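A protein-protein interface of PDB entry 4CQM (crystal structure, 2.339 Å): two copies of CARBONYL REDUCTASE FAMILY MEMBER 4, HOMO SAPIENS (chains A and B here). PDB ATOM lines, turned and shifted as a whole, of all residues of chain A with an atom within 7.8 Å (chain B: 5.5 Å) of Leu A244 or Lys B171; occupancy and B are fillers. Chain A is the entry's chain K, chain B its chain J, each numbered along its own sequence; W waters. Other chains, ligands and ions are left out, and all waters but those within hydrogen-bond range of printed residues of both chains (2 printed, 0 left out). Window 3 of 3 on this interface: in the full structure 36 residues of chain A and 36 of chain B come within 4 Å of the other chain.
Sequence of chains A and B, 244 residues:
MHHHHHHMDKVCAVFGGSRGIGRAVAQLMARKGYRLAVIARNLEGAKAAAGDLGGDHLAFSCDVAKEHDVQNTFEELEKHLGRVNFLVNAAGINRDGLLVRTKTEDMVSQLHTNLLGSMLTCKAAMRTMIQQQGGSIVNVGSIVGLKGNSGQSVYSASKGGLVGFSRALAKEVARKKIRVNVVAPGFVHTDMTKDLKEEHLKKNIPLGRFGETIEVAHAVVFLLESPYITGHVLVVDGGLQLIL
OE1 of Glu B172 is in hydrogen-bond range of N of Gly A151 (3.2 Å).
The backbone carbonyl oxygen (O) of Gly A148 is in hydrogen-bond range of the side-chain amino group (NZ) of Lys B171 (2.6 Å).
The backbone carbonyl oxygen of Lys A147 sits at hydrogen-bond distance from the side-chain amino group of Lys B171 (3.2 Å).
The guanidinium group (NH1) of Arg B167 lies within hydrogen-bond range of the backbone carbonyl oxygen (O) of Leu A146.
NZ of Lys A147 sits at hydrogen-bond distance from O of Gln A241 (2.9 Å).
Lys A147 touches Arg B167 (O to CB, 3.6 Å).
CA of Gly A148 touches N of Ala B168 (3.7 Å).
Ala B168 touches Asn A149 (CB to O, 3.3 Å).
Ser A150 touches Ala B168 (CA to O, 3.9 Å).
Ser A150 touches Glu B172.
Leu A244 touches Lys B171.
Of the printed residues of chain B, Asn A149 touches Ala B168.
Ile A243 touches none of the printed residues of chain B.
Leu A244 touches just one residue of chain B: Lys B171.
No residue of chain A comes within 4 Å of Ala B170.
Lys B171 touches three residues of chain A.
Of the printed residues of chain A, Glu B172 touches Ser A150 (3.3 Å) and Gly A151 (3.2 Å).
The nearest printed residue of chain B that does not touch Leu A244 is Arg B167 (8.9 Å).
The nearest residue of chain A that does not touch Lys B171 is Asn A149 (4.1 Å).
Of the 10 printed residues of chain B, 4 touch a printed residue of chain A.
Hydrophobic or aromatic side chains of chain B within 4 Å of the printed part of chain A: Ala B168.
Of the 20 printed residues of chain A, 7 touch a printed residue of chain B.
Printed residues of chain A that touch a printed residue of chain B: Leu A146, Lys A147, Gly A148, Asn A149, Ser A150, Gly A151 and Leu A244.
Among the printed residues, 10 pairs touch across the chains.
Among the printed residues, no Asp or Glu carboxylate lies within 4 Å of a Lys or Arg side-chain nitrogen of the other chain.
No position is printed for both chains.
Water W2 lies within hydrogen-bond range of O of Leu A244 (2.7 Å), NZ of Lys B171 (3.1 Å) and NZ of Lys A147 (3.5 Å).
Water W1 bridges NZ of Lys B171 (2.9 Å) and OD1 of Asn A149 (2.9 Å).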
ATOM      1  N   SER A 142     -12.725 -26.012  -7.164  1.00  0.00           N
ATOM      2  CA  SER A 142     -12.285 -24.900  -6.328  1.00  0.00           C
ATOM      3  C   SER A 142     -12.943 -23.593  -6.754  1.00  0.00           C
ATOM      4  O   SER A 142     -13.462 -23.482  -7.864  1.00  0.00           O
ATOM      5  CB  SER A 142     -10.762 -24.754  -6.378  1.00  0.00           C
ATOM      6  OG  SER A 142     -10.325 -23.694  -5.544  1.00  0.00           O
ATOM      7  N   ILE A 143     -12.916 -22.606  -5.865  1.00  0.00           N
ATOM      8  CA  ILE A 143     -13.470 -21.292  -6.163  1.00  0.00           C
ATOM      9  C   ILE A 143     -12.592 -20.551  -7.168  1.00  0.00           C
ATOM     10  O   ILE A 143     -13.076 -19.719  -7.935  1.00  0.00           O
ATOM     11  CB  ILE A 143     -13.619 -20.436  -4.891  1.00  0.00           C
ATOM     12  N   VAL A 144     -11.300 -20.865  -7.162  1.00  0.00           N
ATOM     13  CA  VAL A 144     -10.354 -20.236  -8.077  1.00  0.00           C
ATOM     14  C   VAL A 144     -10.487 -20.819  -9.480  1.00  0.00           C
ATOM     15  O   VAL A 144      -9.949 -20.275 -10.443  1.00  0.00           O
ATOM     16  CB  VAL A 144      -8.900 -20.400  -7.593  1.00  0.00           C
ATOM     17  CG1 VAL A 144      -8.764 -19.925  -6.154  1.00  0.00           C
ATOM     18  CG2 VAL A 144      -8.458 -21.847  -7.720  1.00  0.00           C
ATOM     19  N   GLY A 145     -11.205 -21.932  -9.592  1.00  0.00           N
ATOM     20  CA  GLY A 145     -11.475 -22.529 -10.884  1.00  0.00           C
ATOM     21  C   GLY A 145     -12.456 -21.686 -11.675  1.00  0.00           C
ATOM     22  O   GLY A 145     -12.498 -21.748 -12.902  1.00  0.00           O
ATOM     23  N   LEU A 146     -13.245 -20.886 -10.964  1.00  0.00           N
ATOM     24  CA  LEU A 146     -14.242 -20.032 -11.597  1.00  0.00           C
ATOM     25  C   LEU A 146     -13.850 -18.559 -11.580  1.00  0.00           C
ATOM     26  O   LEU A 146     -13.985 -17.867 -12.589  1.00  0.00           O
ATOM     27  CB  LEU A 146     -15.604 -20.210 -10.922  1.00  0.00           C
ATOM     28  CG  LEU A 146     -16.553 -21.214 -11.580  1.00  0.00           C
ATOM     29  CD1 LEU A 146     -17.867 -21.289 -10.817  1.00  0.00           C
ATOM     30  CD2 LEU A 146     -16.795 -20.842 -13.036  1.00  0.00           C
ATOM     31  N   LYS A 147     -13.370 -18.076 -10.439  1.00  0.00           N
ATOM     32  CA  LYS A 147     -13.051 -16.659 -10.298  1.00  0.00           C
ATOM     33  C   LYS A 147     -11.571 -16.367 -10.528  1.00  0.00           C
ATOM     34  O   LYS A 147     -11.180 -15.213 -10.697  1.00  0.00           O
ATOM     35  CB  LYS A 147     -13.467 -16.149  -8.916  1.00  0.00           C
ATOM     36  CG  LYS A 147     -14.947 -16.325  -8.599  1.00  0.00           C
ATOM     37  CD  LYS A 147     -15.452 -15.224  -7.674  1.00  0.00           C
ATOM     38  CE  LYS A 147     -16.125 -14.100  -8.454  1.00  0.00           C
ATOM     39  NZ  LYS A 147     -16.428 -12.920  -7.589  1.00  0.00           N
ATOM     40  N   GLY A 148     -10.750 -17.411 -10.532  1.00  0.00           N
ATOM     41  CA  GLY A 148      -9.327 -17.253 -10.770  1.00  0.00           C
ATOM     42  C   GLY A 148      -8.576 -16.688  -9.579  1.00  0.00           C
ATOM     43  O   GLY A 148      -9.162 -16.045  -8.707  1.00  0.00           O
ATOM     44  N   ASN A 149      -7.271 -16.934  -9.543  1.00  0.00           N
ATOM     45  CA  ASN A 149      -6.421 -16.415  -8.479  1.00  0.00           C
ATOM     46  C   ASN A 149      -4.978 -16.262  -8.950  1.00  0.00           C
ATOM     47  O   ASN A 149      -4.464 -17.106  -9.684  1.00  0.00           O
ATOM     48  CB  ASN A 149      -6.484 -17.327  -7.253  1.00  0.00           C
ATOM     49  CG  ASN A 149      -5.905 -16.675  -6.013  1.00  0.00           C
ATOM     50  OD1 ASN A 149      -5.756 -15.455  -5.950  1.00  0.00           O
ATOM     51  ND2 ASN A 149      -5.579 -17.488  -5.014  1.00  0.00           N
ATOM     52  N   SER A 150      -4.333 -15.180  -8.529  1.00  0.00           N
ATOM     53  CA  SER A 150      -2.964 -14.891  -8.939  1.00  0.00           C
ATOM     54  C   SER A 150      -1.998 -15.967  -8.453  1.00  0.00           C
ATOM     55  O   SER A 150      -2.054 -16.389  -7.298  1.00  0.00           O
ATOM     56  CB  SER A 150      -2.528 -13.520  -8.422  1.00  0.00           C
ATOM     57  OG  SER A 150      -1.218 -13.203  -8.861  1.00  0.00           O
ATOM     58  N   GLY A 151      -1.116 -16.408  -9.345  1.00  0.00           N
ATOM     59  CA  GLY A 151      -0.142 -17.433  -9.017  1.00  0.00           C
ATOM     60  C   GLY A 151      -0.728 -18.832  -9.044  1.00  0.00           C
ATOM     61  O   GLY A 151      -0.078 -19.794  -8.635  1.00  0.00           O
ATOM     62  N   GLY A 186     -13.447 -23.055  -0.856  1.00  0.00           N
ATOM     63  CA  GLY A 186     -12.566 -21.904  -0.840  1.00  0.00           C
ATOM     64  C   GLY A 186     -11.269 -22.237  -0.133  1.00  0.00           C
ATOM     65  O   GLY A 186     -10.606 -23.218  -0.467  1.00  0.00           O
ATOM     66  N   PHE A 187     -10.909 -21.421   0.852  1.00  0.00           N
ATOM     67  CA  PHE A 187      -9.702 -21.658   1.632  1.00  0.00           C
ATOM     68  C   PHE A 187      -9.971 -22.668   2.742  1.00  0.00           C
ATOM     69  O   PHE A 187     -10.643 -22.364   3.728  1.00  0.00           O
ATOM     70  CB  PHE A 187      -9.175 -20.349   2.222  1.00  0.00           C
ATOM     71  CG  PHE A 187      -8.844 -19.306   1.191  1.00  0.00           C
ATOM     72  CD1 PHE A 187      -8.408 -19.671  -0.072  1.00  0.00           C
ATOM     73  CD2 PHE A 187      -8.970 -17.958   1.486  1.00  0.00           C
ATOM     74  CE1 PHE A 187      -8.104 -18.711  -1.021  1.00  0.00           C
ATOM     75  CE2 PHE A 187      -8.668 -16.994   0.543  1.00  0.00           C
ATOM     76  CZ  PHE A 187      -8.234 -17.372  -0.712  1.00  0.00           C
ATOM     77  N   ASN A 204     -10.786 -11.009   5.716  1.00  0.00           N
ATOM     78  CA  ASN A 204     -11.649 -10.631   4.605  1.00  0.00           C
ATOM     79  C   ASN A 204     -12.910 -11.486   4.552  1.00  0.00           C
ATOM     80  O   ASN A 204     -14.018 -10.965   4.431  1.00  0.00           O
ATOM     81  CB  ASN A 204     -10.890 -10.741   3.281  1.00  0.00           C
ATOM     82  CG  ASN A 204      -9.649  -9.872   3.244  1.00  0.00           C
ATOM     83  OD1 ASN A 204      -9.178  -9.397   4.278  1.00  0.00           O
ATOM     84  ND2 ASN A 204      -9.111  -9.659   2.048  1.00  0.00           N
ATOM     85  N   ASP A 237     -17.200 -21.677   0.747  1.00  0.00           N
ATOM     86  CA  ASP A 237     -16.094 -20.741   0.907  1.00  0.00           C
ATOM     87  C   ASP A 237     -16.240 -19.848   2.134  1.00  0.00           C
ATOM     88  O   ASP A 237     -15.254 -19.310   2.639  1.00  0.00           O
ATOM     89  CB  ASP A 237     -15.963 -19.874  -0.343  1.00  0.00           C
ATOM     90  CG  ASP A 237     -17.237 -19.115  -0.657  1.00  0.00           C
ATOM     91  OD1 ASP A 237     -18.327 -19.614  -0.308  1.00  0.00           O
ATOM     92  OD2 ASP A 237     -17.148 -18.021  -1.252  1.00  0.00           O
ATOM     93  N   GLY A 239     -18.380 -17.196   2.087  1.00  0.00           N
ATOM     94  CA  GLY A 239     -18.663 -15.871   1.567  1.00  0.00           C
ATOM     95  C   GLY A 239     -17.482 -15.254   0.846  1.00  0.00           C
ATOM     96  O   GLY A 239     -17.501 -14.071   0.506  1.00  0.00           O
ATOM     97  N   LEU A 240     -16.454 -16.062   0.608  1.00  0.00           N
ATOM     98  CA  LEU A 240     -15.235 -15.593  -0.043  1.00  0.00           C
ATOM     99  C   LEU A 240     -15.485 -15.135  -1.477  1.00  0.00           C
ATOM    100  O   LEU A 240     -14.864 -14.183  -1.949  1.00  0.00           O
ATOM    101  CB  LEU A 240     -14.174 -16.694  -0.029  1.00  0.00           C
ATOM    102  CG  LEU A 240     -12.831 -16.375  -0.688  1.00  0.00           C
ATOM    103  CD1 LEU A 240     -12.065 -15.336   0.120  1.00  0.00           C
ATOM    104  CD2 LEU A 240     -12.008 -17.640  -0.871  1.00  0.00           C
ATOM    105  N   GLN A 241     -16.404 -15.810  -2.165  1.00  0.00           N
ATOM    106  CA  GLN A 241     -16.674 -15.528  -3.574  1.00  0.00           C
ATOM    107  C   GLN A 241     -17.310 -14.158  -3.787  1.00  0.00           C
ATOM    108  O   GLN A 241     -17.344 -13.648  -4.906  1.00  0.00           O
ATOM    109  CB  GLN A 241     -17.576 -16.610  -4.171  1.00  0.00           C
ATOM    110  CG  GLN A 241     -18.963 -16.670  -3.555  1.00  0.00           C
ATOM    111  CD  GLN A 241     -19.882 -17.634  -4.281  1.00  0.00           C
ATOM    112  OE1 GLN A 241     -19.717 -17.886  -5.475  1.00  0.00           O
ATOM    113  NE2 GLN A 241     -20.854 -18.181  -3.562  1.00  0.00           N
ATOM    114  N   LEU A 242     -17.816 -13.567  -2.710  1.00  0.00           N
ATOM    115  CA  LEU A 242     -18.462 -12.264  -2.785  1.00  0.00           C
ATOM    116  C   LEU A 242     -17.435 -11.133  -2.799  1.00  0.00           C
ATOM    117  O   LEU A 242     -17.732 -10.016  -3.224  1.00  0.00           O
ATOM    118  CB  LEU A 242     -19.428 -12.080  -1.611  1.00  0.00           C
ATOM    119  CG  LEU A 242     -20.445 -13.201  -1.379  1.00  0.00           C
ATOM    120  CD1 LEU A 242     -21.339 -12.880  -0.191  1.00  0.00           C
ATOM    121  CD2 LEU A 242     -21.276 -13.451  -2.629  1.00  0.00           C
ATOM    122  N   ILE A 243     -16.227 -11.431  -2.335  1.00  0.00           N
ATOM    123  CA  ILE A 243     -15.186 -10.420  -2.200  1.00  0.00           C
ATOM    124  C   ILE A 243     -13.931 -10.771  -2.992  1.00  0.00           C
ATOM    125  O   ILE A 243     -13.040  -9.937  -3.158  1.00  0.00           O
ATOM    126  CB  ILE A 243     -14.793 -10.226  -0.729  1.00  0.00           C
ATOM    127  CG1 ILE A 243     -14.269 -11.544  -0.157  1.00  0.00           C
ATOM    128  CG2 ILE A 243     -15.978  -9.722   0.078  1.00  0.00           C
ATOM    129  CD1 ILE A 243     -13.828 -11.454   1.271  1.00  0.00           C
ATOM    130  N   LEU A 244     -13.862 -12.010  -3.469  1.00  0.00           N
ATOM    131  CA  LEU A 244     -12.692 -12.488  -4.196  1.00  0.00           C
ATOM    132  C   LEU A 244     -12.498 -11.729  -5.504  1.00  0.00           C
ATOM    133  O   LEU A 244     -13.462 -11.435  -6.209  1.00  0.00           O
ATOM    134  CB  LEU A 244     -12.812 -13.987  -4.473  1.00  0.00           C
ATOM    135  CG  LEU A 244     -11.578 -14.659  -5.080  1.00  0.00           C
ATOM    136  CD1 LEU A 244     -10.407 -14.595  -4.112  1.00  0.00           C
ATOM    137  CD2 LEU A 244     -11.882 -16.098  -5.466  1.00  0.00           C
ATOM    138  N   SER B 166      -7.871 -17.648 -17.743  1.00  0.00           N
ATOM    139  CA  SER B 166      -7.803 -16.260 -18.182  1.00  0.00           C
ATOM    140  C   SER B 166      -8.057 -15.291 -17.034  1.00  0.00           C
ATOM    141  O   SER B 166      -7.510 -14.191 -17.010  1.00  0.00           O
ATOM    142  CB  SER B 166      -8.806 -16.007 -19.306  1.00  0.00           C
ATOM    143  OG  SER B 166      -8.554 -16.855 -20.414  1.00  0.00           O
ATOM    144  N   ARG B 167      -8.886 -15.708 -16.083  1.00  0.00           N
ATOM    145  CA  ARG B 167      -9.197 -14.877 -14.927  1.00  0.00           C
ATOM    146  C   ARG B 167      -8.058 -14.886 -13.913  1.00  0.00           C
ATOM    147  O   ARG B 167      -7.734 -13.856 -13.322  1.00  0.00           O
ATOM    148  CB  ARG B 167     -10.498 -15.341 -14.271  1.00  0.00           C
ATOM    149  CG  ARG B 167     -11.744 -14.932 -15.037  1.00  0.00           C
ATOM    150  CD  ARG B 167     -13.009 -15.421 -14.354  1.00  0.00           C
ATOM    151  NE  ARG B 167     -14.212 -14.919 -15.011  1.00  0.00           N
ATOM    152  CZ  ARG B 167     -15.445 -15.315 -14.716  1.00  0.00           C
ATOM    153  NH1 ARG B 167     -15.642 -16.228 -13.775  1.00  0.00           N
ATOM    154  NH2 ARG B 167     -16.481 -14.802 -15.365  1.00  0.00           N
ATOM    155  N   ALA B 168      -7.454 -16.053 -13.717  1.00  0.00           N
ATOM    156  CA  ALA B 168      -6.321 -16.178 -12.808  1.00  0.00           C
ATOM    157  C   ALA B 168      -5.115 -15.424 -13.353  1.00  0.00           C
ATOM    158  O   ALA B 168      -4.329 -14.854 -12.595  1.00  0.00           O
ATOM    159  CB  ALA B 168      -5.981 -17.639 -12.584  1.00  0.00           C
ATOM    160  N   LEU B 169      -4.976 -15.424 -14.675  1.00  0.00           N
ATOM    161  CA  LEU B 169      -3.900 -14.696 -15.334  1.00  0.00           C
ATOM    162  C   LEU B 169      -4.184 -13.200 -15.332  1.00  0.00           C
ATOM    163  O   LEU B 169      -3.266 -12.386 -15.227  1.00  0.00           O
ATOM    164  CB  LEU B 169      -3.708 -15.195 -16.769  1.00  0.00           C
ATOM    165  CG  LEU B 169      -2.597 -14.519 -17.576  1.00  0.00           C
ATOM    166  CD1 LEU B 169      -1.254 -14.666 -16.873  1.00  0.00           C
ATOM    167  CD2 LEU B 169      -2.531 -15.082 -18.986  1.00  0.00           C
ATOM    168  N   ALA B 170      -5.461 -12.846 -15.446  1.00  0.00           N
ATOM    169  CA  ALA B 170      -5.874 -11.447 -15.435  1.00  0.00           C
ATOM    170  C   ALA B 170      -5.489 -10.781 -14.120  1.00  0.00           C
ATOM    171  O   ALA B 170      -4.943  -9.680 -14.113  1.00  0.00           O
ATOM    172  CB  ALA B 170      -7.370 -11.329 -15.672  1.00  0.00           C
ATOM    173  N   LYS B 171      -5.772 -11.457 -13.013  1.00  0.00           N
ATOM    174  CA  LYS B 171      -5.405 -10.959 -11.693  1.00  0.00           C
ATOM    175  C   LYS B 171      -3.890 -10.911 -11.522  1.00  0.00           C
ATOM    176  O   LYS B 171      -3.354 -10.019 -10.866  1.00  0.00           O
ATOM    177  CB  LYS B 171      -6.015 -11.835 -10.597  1.00  0.00           C
ATOM    178  CG  LYS B 171      -7.531 -11.866 -10.577  1.00  0.00           C
ATOM    179  CD  LYS B 171      -8.031 -12.786  -9.476  1.00  0.00           C
ATOM    180  CE  LYS B 171      -9.539 -12.710  -9.324  1.00  0.00           C
ATOM    181  NZ  LYS B 171     -10.029 -13.603  -8.238  1.00  0.00           N
ATOM    182  N   GLU B 172      -3.212 -11.880 -12.126  1.00  0.00           N
ATOM    183  CA  GLU B 172      -1.778 -12.060 -11.945  1.00  0.00           C
ATOM    184  C   GLU B 172      -0.949 -10.962 -12.612  1.00  0.00           C
ATOM    185  O   GLU B 172       0.142 -10.630 -12.147  1.00  0.00           O
ATOM    186  CB  GLU B 172      -1.360 -13.433 -12.485  1.00  0.00           C
ATOM    187  CG  GLU B 172       0.117 -13.762 -12.333  1.00  0.00           C
ATOM    188  CD  GLU B 172       0.448 -15.173 -12.785  1.00  0.00           C
ATOM    189  OE1 GLU B 172      -0.297 -16.106 -12.420  1.00  0.00           O
ATOM    190  OE2 GLU B 172       1.455 -15.349 -13.503  1.00  0.00           O
ATOM    191  N   VAL B 173      -1.473 -10.385 -13.689  1.00  0.00           N
ATOM    192  CA  VAL B 173      -0.683  -9.471 -14.506  1.00  0.00           C
ATOM    193  C   VAL B 173      -1.416  -8.148 -14.782  1.00  0.00           C
ATOM    194  O   VAL B 173      -1.001  -7.351 -15.627  1.00  0.00           O
ATOM    195  CB  VAL B 173      -0.283 -10.161 -15.839  1.00  0.00           C
ATOM    196  CG1 VAL B 173      -1.449 -10.175 -16.823  1.00  0.00           C
ATOM    197  CG2 VAL B 173       0.964  -9.521 -16.443  1.00  0.00           C
ATOM    198  N   ALA B 174      -2.492  -7.902 -14.041  1.00  0.00           N
ATOM    199  CA  ALA B 174      -3.274  -6.679 -14.209  1.00  0.00           C
ATOM    200  C   ALA B 174      -2.453  -5.424 -13.921  1.00  0.00           C
ATOM    201  O   ALA B 174      -2.665  -4.379 -14.538  1.00  0.00           O
ATOM    202  CB  ALA B 174      -4.504  -6.711 -13.316  1.00  0.00           C
ATOM    203  N   ARG B 175      -1.514  -5.531 -12.985  1.00  0.00           N
ATOM    204  CA  ARG B 175      -0.692  -4.389 -12.593  1.00  0.00           C
ATOM    205  C   ARG B 175       0.364  -4.061 -13.642  1.00  0.00           C
ATOM    206  O   ARG B 175       0.965  -2.987 -13.614  1.00  0.00           O
ATOM    207  CB  ARG B 175      -0.028  -4.652 -11.240  1.00  0.00           C
ATOM    208  CG  ARG B 175      -1.005  -4.649 -10.076  1.00  0.00           C
ATOM    209  CD  ARG B 175      -1.727  -3.314  -9.986  1.00  0.00           C
ATOM    210  NE  ARG B 175      -2.972  -3.406  -9.231  1.00  0.00           N
ATOM    211  CZ  ARG B 175      -3.091  -3.112  -7.940  1.00  0.00           C
ATOM    212  NH1 ARG B 175      -2.034  -2.703  -7.250  1.00  0.00           N
ATOM    213  NH2 ARG B 175      -4.268  -3.226  -7.339  1.00  0.00           N
HETATM  214  O   HOH W   1      -8.031 -13.651  -6.187  1.00  0.00           O
HETATM  215  O   HOH W   2     -13.052 -12.835  -8.426  1.00  0.00           O
